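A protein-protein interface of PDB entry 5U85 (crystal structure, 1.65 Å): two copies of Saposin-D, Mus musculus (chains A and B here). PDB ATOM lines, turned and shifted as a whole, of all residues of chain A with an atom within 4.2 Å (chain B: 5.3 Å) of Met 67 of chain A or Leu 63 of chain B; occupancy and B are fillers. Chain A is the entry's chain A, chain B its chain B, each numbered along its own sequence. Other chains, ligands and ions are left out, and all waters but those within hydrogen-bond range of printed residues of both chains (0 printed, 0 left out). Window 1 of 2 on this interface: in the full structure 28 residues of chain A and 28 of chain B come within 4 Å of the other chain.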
ATOM      1  N   VAL A  13      -1.111 -37.812  -2.843  1.00  0.00           N
ATOM      2  CA  VAL A  13      -0.909 -36.369  -2.938  1.00  0.00           C
ATOM      3  C   VAL A  13      -1.688 -35.800  -4.117  1.00  0.00           C
ATOM      4  O   VAL A  13      -2.200 -34.676  -4.046  1.00  0.00           O
ATOM      5  CB  VAL A  13       0.593 -36.035  -3.029  1.00  0.00           C
ATOM      6  CG1 VAL A  13       0.798 -34.529  -3.155  1.00  0.00           C
ATOM      7  CG2 VAL A  13       1.330 -36.554  -1.800  1.00  0.00           C
ATOM      8  N   LEU A  16      -5.049 -35.285  -2.770  1.00  0.00           N
ATOM      9  CA  LEU A  16      -5.125 -34.125  -1.887  1.00  0.00           C
ATOM     10  C   LEU A  16      -5.080 -32.830  -2.683  1.00  0.00           C
ATOM     11  O   LEU A  16      -5.783 -31.865  -2.359  1.00  0.00           O
ATOM     12  CB  LEU A  16      -3.981 -34.164  -0.873  1.00  0.00           C
ATOM     13  CG  LEU A  16      -3.969 -35.331   0.118  1.00  0.00           C
ATOM     14  CD1 LEU A  16      -2.681 -35.311   0.921  1.00  0.00           C
ATOM     15  CD2 LEU A  16      -5.174 -35.277   1.041  1.00  0.00           C
ATOM     16  N   GLU A  17      -4.242 -32.794  -3.718  1.00  0.00           N
ATOM     17  CA  GLU A  17      -4.163 -31.628  -4.589  1.00  0.00           C
ATOM     18  C   GLU A  17      -5.530 -31.292  -5.177  1.00  0.00           C
ATOM     19  O   GLU A  17      -5.968 -30.136  -5.148  1.00  0.00           O
ATOM     20  CB  GLU A  17      -3.138 -31.917  -5.687  1.00  0.00           C
ATOM     21  CG  GLU A  17      -2.809 -30.782  -6.630  1.00  0.00           C
ATOM     22  CD  GLU A  17      -1.809 -31.214  -7.686  1.00  0.00           C
ATOM     23  OE1 GLU A  17      -1.921 -32.361  -8.172  1.00  0.00           O
ATOM     24  OE2 GLU A  17      -0.903 -30.422  -8.018  1.00  0.00           O
ATOM     25  N   LEU A  20      -8.317 -30.102  -2.668  1.00  0.00           N
ATOM     26  CA  LEU A  20      -8.293 -28.688  -2.311  1.00  0.00           C
ATOM     27  C   LEU A  20      -9.154 -27.853  -3.250  1.00  0.00           C
ATOM     28  O   LEU A  20      -9.565 -26.749  -2.878  1.00  0.00           O
ATOM     29  CB  LEU A  20      -6.855 -28.162  -2.320  1.00  0.00           C
ATOM     30  CG  LEU A  20      -5.909 -28.625  -1.209  1.00  0.00           C
ATOM     31  CD1 LEU A  20      -4.477 -28.251  -1.559  1.00  0.00           C
ATOM     32  CD2 LEU A  20      -6.288 -28.031   0.141  1.00  0.00           C
ATOM     33  N   LEU A  63      -1.149 -23.044  -1.263  1.00  0.00           N
ATOM     34  CA  LEU A  63      -1.282 -24.383  -0.700  1.00  0.00           C
ATOM     35  C   LEU A  63      -1.396 -25.433  -1.799  1.00  0.00           C
ATOM     36  O   LEU A  63      -0.781 -26.503  -1.712  1.00  0.00           O
ATOM     37  CB  LEU A  63      -2.492 -24.438   0.229  1.00  0.00           C
ATOM     38  CG  LEU A  63      -2.753 -25.773   0.930  1.00  0.00           C
ATOM     39  CD1 LEU A  63      -1.546 -26.210   1.750  1.00  0.00           C
ATOM     40  CD2 LEU A  63      -3.986 -25.649   1.804  1.00  0.00           C
ATOM     41  N   VAL A  64      -2.177 -25.148  -2.842  1.00  0.00           N
ATOM     42  CA  VAL A  64      -2.281 -26.076  -3.965  1.00  0.00           C
ATOM     43  C   VAL A  64      -0.914 -26.290  -4.604  1.00  0.00           C
ATOM     44  O   VAL A  64      -0.541 -27.421  -4.943  1.00  0.00           O
ATOM     45  CB  VAL A  64      -3.318 -25.566  -4.985  1.00  0.00           C
ATOM     46  CG1 VAL A  64      -3.339 -26.447  -6.229  1.00  0.00           C
ATOM     47  CG2 VAL A  64      -4.703 -25.518  -4.353  1.00  0.00           C
ATOM     48  N   GLU A  65      -0.140 -25.212  -4.772  1.00  0.00           N
ATOM     49  CA  GLU A  65       1.174 -25.333  -5.400  1.00  0.00           C
ATOM     50  C   GLU A  65       2.108 -26.214  -4.579  1.00  0.00           C
ATOM     51  O   GLU A  65       2.915 -26.965  -5.140  1.00  0.00           O
ATOM     52  CB  GLU A  65       1.789 -23.948  -5.601  1.00  0.00           C
ATOM     53  CG  GLU A  65       1.038 -23.098  -6.609  1.00  0.00           C
ATOM     54  CD  GLU A  65       1.649 -21.723  -6.801  1.00  0.00           C
ATOM     55  OE1 GLU A  65       2.225 -21.181  -5.835  1.00  0.00           O
ATOM     56  OE2 GLU A  65       1.549 -21.184  -7.923  1.00  0.00           O
ATOM     57  N   VAL A  66       2.024 -26.130  -3.250  1.00  0.00           N
ATOM     58  CA  VAL A  66       2.866 -26.968  -2.402  1.00  0.00           C
ATOM     59  C   VAL A  66       2.465 -28.430  -2.535  1.00  0.00           C
ATOM     60  O   VAL A  66       3.315 -29.326  -2.448  1.00  0.00           O
ATOM     61  CB  VAL A  66       2.787 -26.490  -0.939  1.00  0.00           C
ATOM     62  CG1 VAL A  66       3.494 -27.466   0.000  1.00  0.00           C
ATOM     63  CG2 VAL A  66       3.391 -25.104  -0.807  1.00  0.00           C
ATOM     64  N   MET A  67       1.180 -28.697  -2.756  1.00  0.00           N
ATOM     65  CA  MET A  67       0.661 -30.058  -2.806  1.00  0.00           C
ATOM     66  C   MET A  67       0.952 -30.716  -4.151  1.00  0.00           C
ATOM     67  O   MET A  67       0.038 -31.227  -4.807  1.00  0.00           O
ATOM     68  CB  MET A  67      -0.845 -30.042  -2.530  1.00  0.00           C
ATOM     69  CG  MET A  67      -1.410 -31.349  -1.998  1.00  0.00           C
ATOM     70  SD  MET A  67      -0.721 -31.820  -0.398  1.00  0.00           S
ATOM     71  CE  MET A  67      -1.190 -30.421   0.619  1.00  0.00           C
ATOM     72  N   ASP A  68       2.221 -30.715  -4.568  1.00  0.00           N
ATOM     73  CA  ASP A  68       2.628 -31.346  -5.816  1.00  0.00           C
ATOM     74  C   ASP A  68       3.148 -32.746  -5.527  1.00  0.00           C
ATOM     75  O   ASP A  68       4.072 -32.886  -4.712  1.00  0.00           O
ATOM     76  CB  ASP A  68       3.704 -30.517  -6.509  1.00  0.00           C
ATOM     77  CG  ASP A  68       4.348 -31.251  -7.671  1.00  0.00           C
ATOM     78  OD1 ASP A  68       3.717 -31.338  -8.745  1.00  0.00           O
ATOM     79  OD2 ASP A  68       5.489 -31.736  -7.511  1.00  0.00           O
ATOM     80  N   PRO A  69       2.606 -33.799  -6.153  1.00  0.00           N
ATOM     81  CA  PRO A  69       3.036 -35.163  -5.788  1.00  0.00           C
ATOM     82  C   PRO A  69       4.542 -35.379  -5.794  1.00  0.00           C
ATOM     83  O   PRO A  69       5.086 -35.927  -4.827  1.00  0.00           O
ATOM     84  CB  PRO A  69       2.320 -36.027  -6.833  1.00  0.00           C
ATOM     85  CG  PRO A  69       1.088 -35.266  -7.145  1.00  0.00           C
ATOM     86  CD  PRO A  69       1.506 -33.823  -7.134  1.00  0.00           C
ATOM     87  N   GLU B  17      -1.711 -23.324  11.576  1.00  0.00           N
ATOM     88  CA  GLU B  17      -0.719 -24.367  11.796  1.00  0.00           C
ATOM     89  C   GLU B  17      -0.772 -24.888  13.229  1.00  0.00           C
ATOM     90  O   GLU B  17      -0.659 -26.097  13.457  1.00  0.00           O
ATOM     91  CB  GLU B  17       0.661 -23.833  11.417  1.00  0.00           C
ATOM     92  CG  GLU B  17       0.759 -23.626   9.906  1.00  0.00           C
ATOM     93  CD  GLU B  17       2.009 -22.904   9.450  1.00  0.00           C
ATOM     94  OE1 GLU B  17       2.719 -22.318  10.292  1.00  0.00           O
ATOM     95  OE2 GLU B  17       2.276 -22.924   8.229  1.00  0.00           O
ATOM     96  N   LEU B  58       5.126 -36.797   9.402  1.00  0.00           N
ATOM     97  CA  LEU B  58       6.142 -36.119   8.605  1.00  0.00           C
ATOM     98  C   LEU B  58       5.501 -35.286   7.500  1.00  0.00           C
ATOM     99  O   LEU B  58       5.989 -34.199   7.173  1.00  0.00           O
ATOM    100  CB  LEU B  58       7.123 -37.136   8.019  1.00  0.00           C
ATOM    101  CG  LEU B  58       8.349 -36.568   7.294  1.00  0.00           C
ATOM    102  CD1 LEU B  58       9.173 -35.659   8.199  1.00  0.00           C
ATOM    103  CD2 LEU B  58       9.222 -37.692   6.751  1.00  0.00           C
ATOM    104  N   LEU B  59       4.405 -35.776   6.917  1.00  0.00           N
ATOM    105  CA  LEU B  59       3.688 -34.988   5.917  1.00  0.00           C
ATOM    106  C   LEU B  59       3.286 -33.634   6.482  1.00  0.00           C
ATOM    107  O   LEU B  59       3.540 -32.590   5.868  1.00  0.00           O
ATOM    108  CB  LEU B  59       2.458 -35.755   5.427  1.00  0.00           C
ATOM    109  CG  LEU B  59       2.711 -36.848   4.387  1.00  0.00           C
ATOM    110  CD1 LEU B  59       1.490 -37.744   4.251  1.00  0.00           C
ATOM    111  CD2 LEU B  59       3.072 -36.237   3.041  1.00  0.00           C
ATOM    112  N   LEU B  60       2.661 -33.624   7.663  1.00  0.00           N
ATOM    113  CA  LEU B  60       2.248 -32.363   8.270  1.00  0.00           C
ATOM    114  C   LEU B  60       3.449 -31.505   8.643  1.00  0.00           C
ATOM    115  O   LEU B  60       3.419 -30.281   8.472  1.00  0.00           O
ATOM    116  CB  LEU B  60       1.384 -32.625   9.503  1.00  0.00           C
ATOM    117  CG  LEU B  60      -0.021 -33.182   9.273  1.00  0.00           C
ATOM    118  CD1 LEU B  60      -0.716 -33.367  10.610  1.00  0.00           C
ATOM    119  CD2 LEU B  60      -0.838 -32.265   8.369  1.00  0.00           C
ATOM    120  N   GLU B  61       4.510 -32.123   9.168  1.00  0.00           N
ATOM    121  CA  GLU B  61       5.699 -31.358   9.530  1.00  0.00           C
ATOM    122  C   GLU B  61       6.300 -30.671   8.310  1.00  0.00           C
ATOM    123  O   GLU B  61       6.699 -29.503   8.378  1.00  0.00           O
ATOM    124  CB  GLU B  61       6.729 -32.273  10.192  1.00  0.00           C
ATOM    125  CG  GLU B  61       6.298 -32.824  11.540  1.00  0.00           C
ATOM    126  CD  GLU B  61       7.266 -33.857  12.081  1.00  0.00           C
ATOM    127  OE1 GLU B  61       7.683 -34.747  11.311  1.00  0.00           O
ATOM    128  OE2 GLU B  61       7.616 -33.775  13.276  1.00  0.00           O
ATOM    129  N   ILE B  62       6.368 -31.380   7.184  1.00  0.00           N
ATOM    130  CA  ILE B  62       6.935 -30.800   5.970  1.00  0.00           C
ATOM    131  C   ILE B  62       6.040 -29.685   5.439  1.00  0.00           C
ATOM    132  O   ILE B  62       6.529 -28.646   4.980  1.00  0.00           O
ATOM    133  CB  ILE B  62       7.167 -31.905   4.922  1.00  0.00           C
ATOM    134  CG1 ILE B  62       8.289 -32.846   5.384  1.00  0.00           C
ATOM    135  CG2 ILE B  62       7.476 -31.313   3.547  1.00  0.00           C
ATOM    136  CD1 ILE B  62       9.665 -32.194   5.495  1.00  0.00           C
ATOM    137  N   LEU B  63       4.721 -29.878   5.487  1.00  0.00           N
ATOM    138  CA  LEU B  63       3.822 -28.841   4.994  1.00  0.00           C
ATOM    139  C   LEU B  63       3.944 -27.567   5.823  1.00  0.00           C
ATOM    140  O   LEU B  63       3.981 -26.464   5.265  1.00  0.00           O
ATOM    141  CB  LEU B  63       2.384 -29.358   4.983  1.00  0.00           C
ATOM    142  CG  LEU B  63       2.117 -30.471   3.962  1.00  0.00           C
ATOM    143  CD1 LEU B  63       0.763 -31.117   4.205  1.00  0.00           C
ATOM    144  CD2 LEU B  63       2.200 -29.945   2.532  1.00  0.00           C
ATOM    145  N   VAL B  64       4.017 -27.693   7.149  1.00  0.00           N
ATOM    146  CA  VAL B  64       4.183 -26.520   8.005  1.00  0.00           C
ATOM    147  C   VAL B  64       5.526 -25.859   7.731  1.00  0.00           C
ATOM    148  O   VAL B  64       5.643 -24.627   7.695  1.00  0.00           O
ATOM    149  CB  VAL B  64       4.036 -26.925   9.483  1.00  0.00           C
ATOM    150  CG1 VAL B  64       4.500 -25.808  10.418  1.00  0.00           C
ATOM    151  CG2 VAL B  64       2.594 -27.308   9.779  1.00  0.00           C
ATOM    152  N   GLU B  65       6.562 -26.675   7.540  1.00  0.00           N
ATOM    153  CA  GLU B  65       7.894 -26.169   7.233  1.00  0.00           C
ATOM    154  C   GLU B  65       7.878 -25.307   5.974  1.00  0.00           C
ATOM    155  O   GLU B  65       8.415 -24.193   5.961  1.00  0.00           O
ATOM    156  CB  GLU B  65       8.835 -27.365   7.079  1.00  0.00           C
ATOM    157  CG  GLU B  65      10.289 -27.070   6.792  1.00  0.00           C
ATOM    158  CD  GLU B  65      11.064 -28.348   6.526  1.00  0.00           C
ATOM    159  OE1 GLU B  65      11.429 -28.595   5.357  1.00  0.00           O
ATOM    160  OE2 GLU B  65      11.279 -29.121   7.484  1.00  0.00           O
ATOM    161  N   VAL B  66       7.255 -25.807   4.905  1.00  0.00           N
ATOM    162  CA  VAL B  66       7.199 -25.059   3.653  1.00  0.00           C
ATOM    163  C   VAL B  66       6.329 -23.817   3.808  1.00  0.00           C
ATOM    164  O   VAL B  66       6.654 -22.745   3.280  1.00  0.00           O
ATOM    165  CB  VAL B  66       6.692 -25.971   2.519  1.00  0.00           C
ATOM    166  CG1 VAL B  66       6.511 -25.189   1.224  1.00  0.00           C
ATOM    167  CG2 VAL B  66       7.656 -27.129   2.305  1.00  0.00           C
ATOM    168  N   MET B  67       5.215 -23.935   4.528  1.00  0.00           N
ATOM    169  CA  MET B  67       4.291 -22.819   4.694  1.00  0.00           C
ATOM    170  C   MET B  67       4.723 -21.926   5.853  1.00  0.00           C
ATOM    171  O   MET B  67       3.930 -21.634   6.754  1.00  0.00           O
ATOM    172  CB  MET B  67       2.869 -23.344   4.906  1.00  0.00           C
ATOM    173  CG  MET B  67       2.332 -24.139   3.719  1.00  0.00           C
ATOM    174  SD  MET B  67       1.978 -23.117   2.272  1.00  0.00           S
ATOM    175  CE  MET B  67       0.506 -22.243   2.793  1.00  0.00           C
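Of the printed residues of chain B, Met 67 of chain A touches Leu 63 (3.9 Å).
Of the printed residues of chain A, Leu 63 of chain B touches Val 66 (3.8 Å) and Met 67 (3.9 Å).
Of the printed residues of chain A, Val 66 of chain B touches Val 66 (3.7 Å).
Of the printed residues of chain A, Met 67 of chain B touches Val 66.
Of the printed residues of chain B, Val 66 of chain A touches Leu 63 (3.8 Å), Val 66 (3.7 Å) and Met 67 (3.9 Å).
Leu 16 of chain A touches none of the printed residues of chain B.
Pro 69 of chain A touches none of the printed residues of chain B.
Leu 63 of chain B touches Val 66 of chain A.
Val 66 of chain A touches Val 66 of chain B (CG2 to CG1, 3.7 Å).
Met 67 of chain B touches Val 66 of chain A.
Met 67 of chain A touches Leu 63 of chain B (CE to CD2, 3.9 Å).
OE2 of Glu 17 of chain B sits close to O of Met 67 of chain B (2.6 Å).
Of the 11 printed residues of chain A, 2 touch a printed residue of chain B.
Printed residues of chain A that touch a printed residue of chain B: Val 66 and Met 67.
Of the 11 printed residues of chain B, 3 touch a printed residue of chain A.
Hydrophobic or aromatic side chains of chain B that line the printed part of chain A: Leu 63, Val 66 and Met 67.
Among the printed residues, no Asp or Glu carboxylate lies within 4 Å of a Lys or Arg side-chain nitrogen of the other chain.
Val 66 of chain A touches Leu 63 of chain B, but with the chains exchanged Leu 63 of chain A does not touch Val 66 of chain B (8.0 Å).
Val 66 of chain A touches its own counterpart, Val 66 of chain B.
Val 66 of chain A touches Met 67 of chain B, but with the chains exchanged Met 67 of chain A does not touch Val 66 of chain B (7.5 Å).
Met 67 of chain A touches Leu 63 of chain B, but with the chains exchanged Leu 63 of chain A does not touch Met 67 of chain B (4.5 Å).
Positions printed for both chains: 17, 63, 64, 65, 66 and 67.
Of the 4 pairs that touch across the chains among the printed residues, 1 has its exchanged pair printed and touching as well.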
